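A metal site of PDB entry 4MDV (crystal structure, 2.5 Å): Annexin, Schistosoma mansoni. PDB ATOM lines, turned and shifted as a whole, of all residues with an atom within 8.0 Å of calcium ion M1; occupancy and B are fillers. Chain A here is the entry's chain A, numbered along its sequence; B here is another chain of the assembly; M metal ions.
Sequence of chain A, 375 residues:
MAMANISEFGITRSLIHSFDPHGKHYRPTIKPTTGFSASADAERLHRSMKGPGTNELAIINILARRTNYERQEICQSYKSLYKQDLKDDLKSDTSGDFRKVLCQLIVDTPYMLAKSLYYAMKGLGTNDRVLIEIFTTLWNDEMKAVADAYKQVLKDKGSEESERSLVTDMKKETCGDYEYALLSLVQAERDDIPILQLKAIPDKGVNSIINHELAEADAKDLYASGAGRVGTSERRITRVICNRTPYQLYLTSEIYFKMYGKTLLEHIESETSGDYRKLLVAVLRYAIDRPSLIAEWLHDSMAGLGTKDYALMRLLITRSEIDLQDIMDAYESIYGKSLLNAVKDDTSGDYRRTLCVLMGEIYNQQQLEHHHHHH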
ATOM      1  N   VAL A 167       5.132  24.150   2.681  1.00  0.00           N
ATOM      2  CA  VAL A 167       6.324  23.538   3.234  1.00  0.00           C
ATOM      3  C   VAL A 167       7.331  24.618   3.594  1.00  0.00           C
ATOM      4  O   VAL A 167       7.955  24.547   4.650  1.00  0.00           O
ATOM      5  CB  VAL A 167       6.911  22.508   2.310  1.00  0.00           C
ATOM      6  CG1 VAL A 167       7.666  21.481   3.139  1.00  0.00           C
ATOM      7  CG2 VAL A 167       5.775  21.851   1.520  1.00  0.00           C
ATOM      8  N   THR A 168       7.476  25.627   2.729  1.00  0.00           N
ATOM      9  CA  THR A 168       8.308  26.776   3.055  1.00  0.00           C
ATOM     10  C   THR A 168       7.956  27.321   4.434  1.00  0.00           C
ATOM     11  O   THR A 168       8.820  27.413   5.320  1.00  0.00           O
ATOM     12  CB  THR A 168       8.180  27.895   2.001  1.00  0.00           C
ATOM     13  OG1 THR A 168       9.103  27.637   0.932  1.00  0.00           O
ATOM     14  CG2 THR A 168       8.484  29.281   2.620  1.00  0.00           C
ATOM     15  N   ASP A 169       6.685  27.664   4.624  1.00  0.00           N
ATOM     16  CA  ASP A 169       6.233  28.171   5.929  1.00  0.00           C
ATOM     17  C   ASP A 169       6.459  27.215   7.097  1.00  0.00           C
ATOM     18  O   ASP A 169       6.912  27.660   8.159  1.00  0.00           O
ATOM     19  CB  ASP A 169       4.769  28.641   5.881  1.00  0.00           C
ATOM     20  CG  ASP A 169       4.624  30.034   5.232  1.00  0.00           C
ATOM     21  OD1 ASP A 169       5.609  30.516   4.640  1.00  0.00           O
ATOM     22  OD2 ASP A 169       3.538  30.636   5.316  1.00  0.00           O
ATOM     23  N   MET A 170       6.183  25.917   6.910  1.00  0.00           N
ATOM     24  CA  MET A 170       6.409  24.943   7.972  1.00  0.00           C
ATOM     25  C   MET A 170       7.866  24.803   8.349  1.00  0.00           C
ATOM     26  O   MET A 170       8.203  24.787   9.532  1.00  0.00           O
ATOM     27  CB  MET A 170       5.916  23.561   7.580  1.00  0.00           C
ATOM     28  CG  MET A 170       4.448  23.425   7.392  1.00  0.00           C
ATOM     29  SD  MET A 170       4.162  21.721   6.936  1.00  0.00           S
ATOM     30  CE  MET A 170       4.840  20.883   8.369  1.00  0.00           C
ATOM     31  N   LYS A 171       8.734  24.650   7.352  1.00  0.00           N
ATOM     32  CA  LYS A 171      10.162  24.502   7.592  1.00  0.00           C
ATOM     33  C   LYS A 171      10.668  25.606   8.514  1.00  0.00           C
ATOM     34  O   LYS A 171      11.380  25.347   9.494  1.00  0.00           O
ATOM     35  CB  LYS A 171      10.940  24.524   6.273  1.00  0.00           C
ATOM     36  CG  LYS A 171      12.451  24.515   6.452  1.00  0.00           C
ATOM     37  CD  LYS A 171      13.183  25.044   5.216  1.00  0.00           C
ATOM     38  CE  LYS A 171      14.608  25.506   5.559  1.00  0.00           C
ATOM     39  NZ  LYS A 171      15.432  25.869   4.369  1.00  0.00           N
ATOM     40  N   LYS A 172      10.292  26.844   8.183  1.00  0.00           N
ATOM     41  CA  LYS A 172      10.684  28.013   8.969  1.00  0.00           C
ATOM     42  C   LYS A 172      10.039  27.961  10.354  1.00  0.00           C
ATOM     43  O   LYS A 172      10.604  28.428  11.351  1.00  0.00           O
ATOM     44  CB  LYS A 172      10.302  29.318   8.257  1.00  0.00           C
ATOM     45  N   GLU A 173       8.862  27.356  10.393  1.00  0.00           N
ATOM     46  CA  GLU A 173       8.014  27.321  11.567  1.00  0.00           C
ATOM     47  C   GLU A 173       8.395  26.193  12.527  1.00  0.00           C
ATOM     48  O   GLU A 173       8.075  26.239  13.720  1.00  0.00           O
ATOM     49  CB  GLU A 173       6.578  27.120  11.093  1.00  0.00           C
ATOM     50  CG  GLU A 173       5.526  27.568  12.056  1.00  0.00           C
ATOM     51  CD  GLU A 173       5.571  29.052  12.289  1.00  0.00           C
ATOM     52  OE1 GLU A 173       6.104  29.764  11.417  1.00  0.00           O
ATOM     53  OE2 GLU A 173       5.077  29.506  13.335  1.00  0.00           O
ATOM     54  N   THR A 174       9.089  25.191  12.006  1.00  0.00           N
ATOM     55  CA  THR A 174       9.236  23.929  12.712  1.00  0.00           C
ATOM     56  C   THR A 174      10.662  23.320  12.659  1.00  0.00           C
ATOM     57  O   THR A 174      11.483  23.704  11.816  1.00  0.00           O
ATOM     58  CB  THR A 174       8.166  22.942  12.236  1.00  0.00           C
ATOM     59  OG1 THR A 174       7.981  21.905  13.206  1.00  0.00           O
ATOM     60  CG2 THR A 174       8.540  22.356  10.881  1.00  0.00           C
ATOM     61  N   CYS A 175      10.931  22.388  13.569  1.00  0.00           N
ATOM     62  CA  CYS A 175      12.274  21.818  13.737  1.00  0.00           C
ATOM     63  C   CYS A 175      12.213  20.435  14.406  1.00  0.00           C
ATOM     64  O   CYS A 175      11.155  20.032  14.908  1.00  0.00           O
ATOM     65  CB  CYS A 175      13.152  22.749  14.580  1.00  0.00           C
ATOM     66  SG  CYS A 175      12.457  23.107  16.216  1.00  0.00           S
ATOM     67  N   GLY A 176      13.360  19.750  14.403  1.00  0.00           N
ATOM     68  CA  GLY A 176      13.533  18.465  15.071  1.00  0.00           C
ATOM     69  C   GLY A 176      12.727  17.286  14.525  1.00  0.00           C
ATOM     70  O   GLY A 176      12.315  17.280  13.355  1.00  0.00           O
ATOM     71  N   GLU A 179       9.396  18.224  13.109  1.00  0.00           N
ATOM     72  CA  GLU A 179       9.432  18.816  11.776  1.00  0.00           C
ATOM     73  C   GLU A 179       9.496  17.724  10.727  1.00  0.00           C
ATOM     74  O   GLU A 179       8.742  17.730   9.754  1.00  0.00           O
ATOM     75  CB  GLU A 179      10.662  19.711  11.636  1.00  0.00           C
ATOM     76  CG  GLU A 179      11.024  20.065  10.211  1.00  0.00           C
ATOM     77  CD  GLU A 179      12.335  20.826  10.137  1.00  0.00           C
ATOM     78  OE1 GLU A 179      12.279  22.073   9.998  1.00  0.00           O
ATOM     79  OE2 GLU A 179      13.416  20.181  10.226  1.00  0.00           O
ATOM     80  N   TYR A 180      10.409  16.786  10.942  1.00  0.00           N
ATOM     81  CA  TYR A 180      10.610  15.710  10.014  1.00  0.00           C
ATOM     82  C   TYR A 180       9.296  14.964   9.776  1.00  0.00           C
ATOM     83  O   TYR A 180       8.911  14.697   8.622  1.00  0.00           O
ATOM     84  CB  TYR A 180      11.690  14.774  10.554  1.00  0.00           C
ATOM     85  CG  TYR A 180      12.107  13.744   9.546  1.00  0.00           C
ATOM     86  CD1 TYR A 180      11.346  12.589   9.333  1.00  0.00           C
ATOM     87  CD2 TYR A 180      13.258  13.925   8.772  1.00  0.00           C
ATOM     88  CE1 TYR A 180      11.722  11.639   8.393  1.00  0.00           C
ATOM     89  CE2 TYR A 180      13.651  12.974   7.834  1.00  0.00           C
ATOM     90  CZ  TYR A 180      12.881  11.830   7.651  1.00  0.00           C
ATOM     91  OH  TYR A 180      13.263  10.887   6.714  1.00  0.00           O
ATOM     92  N   LEU A 183       6.838  17.151   7.857  1.00  0.00           N
ATOM     93  CA  LEU A 183       7.225  17.240   6.461  1.00  0.00           C
ATOM     94  C   LEU A 183       6.876  15.946   5.729  1.00  0.00           C
ATOM     95  O   LEU A 183       6.445  15.961   4.590  1.00  0.00           O
ATOM     96  CB  LEU A 183       8.710  17.588   6.308  1.00  0.00           C
ATOM     97  CG  LEU A 183       9.118  18.898   7.001  1.00  0.00           C
ATOM     98  CD1 LEU A 183      10.464  19.395   6.491  1.00  0.00           C
ATOM     99  CD2 LEU A 183       8.041  19.970   6.817  1.00  0.00           C
ATOM    100  N   THR B 174      15.487  23.083  19.636  1.00  0.00           N
ATOM    101  CA  THR B 174      14.507  24.176  19.663  1.00  0.00           C
ATOM    102  C   THR B 174      14.571  25.132  18.475  1.00  0.00           C
ATOM    103  O   THR B 174      15.611  25.268  17.835  1.00  0.00           O
ATOM    104  CB  THR B 174      14.665  24.989  20.959  1.00  0.00           C
ATOM    105  OG1 THR B 174      14.652  24.104  22.089  1.00  0.00           O
ATOM    106  CG2 THR B 174      13.553  25.980  21.096  1.00  0.00           C
ATOM    107  N   CYS B 175      13.457  25.818  18.191  1.00  0.00           N
ATOM    108  CA  CYS B 175      13.347  26.722  17.038  1.00  0.00           C
ATOM    109  C   CYS B 175      12.291  27.799  17.260  1.00  0.00           C
ATOM    110  O   CYS B 175      11.514  27.743  18.236  1.00  0.00           O
ATOM    111  CB  CYS B 175      12.994  25.965  15.751  1.00  0.00           C
ATOM    112  SG  CYS B 175      11.507  24.893  15.864  1.00  0.00           S
ATOM    113  N   GLY B 176      12.267  28.776  16.355  1.00  0.00           N
ATOM    114  CA  GLY B 176      11.251  29.807  16.333  1.00  0.00           C
ATOM    115  C   GLY B 176      11.245  30.779  17.505  1.00  0.00           C
ATOM    116  O   GLY B 176      12.263  30.989  18.177  1.00  0.00           O
HETATM  117 CA    CA M   1      13.469  24.121  10.354  1.00  0.00          CA
HETATM  118 CA    CA M   2      17.729  26.217  16.766  1.00  0.00          CA
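The side-chain sulfur (SG) of Cys 175 of chain A forms a disulfide with the side-chain sulfur (SG) of Cys 175 of chain B.
OE1 of Glu 179 binds calcium ion M1, at 2.4 Å.
O of Thr 174 of chain A binds calcium ion M1, at 2.5 Å.
O of Lys 171 binds calcium ion M1.
Calcium ion M1 has three donor atoms within binding distance.
Of the 16 residues printed, 3 come within 4 Å of calcium ion M1.
The nearest printed residue that does not touch calcium ion M1 is Cys 175 of chain A (4.3 Å).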
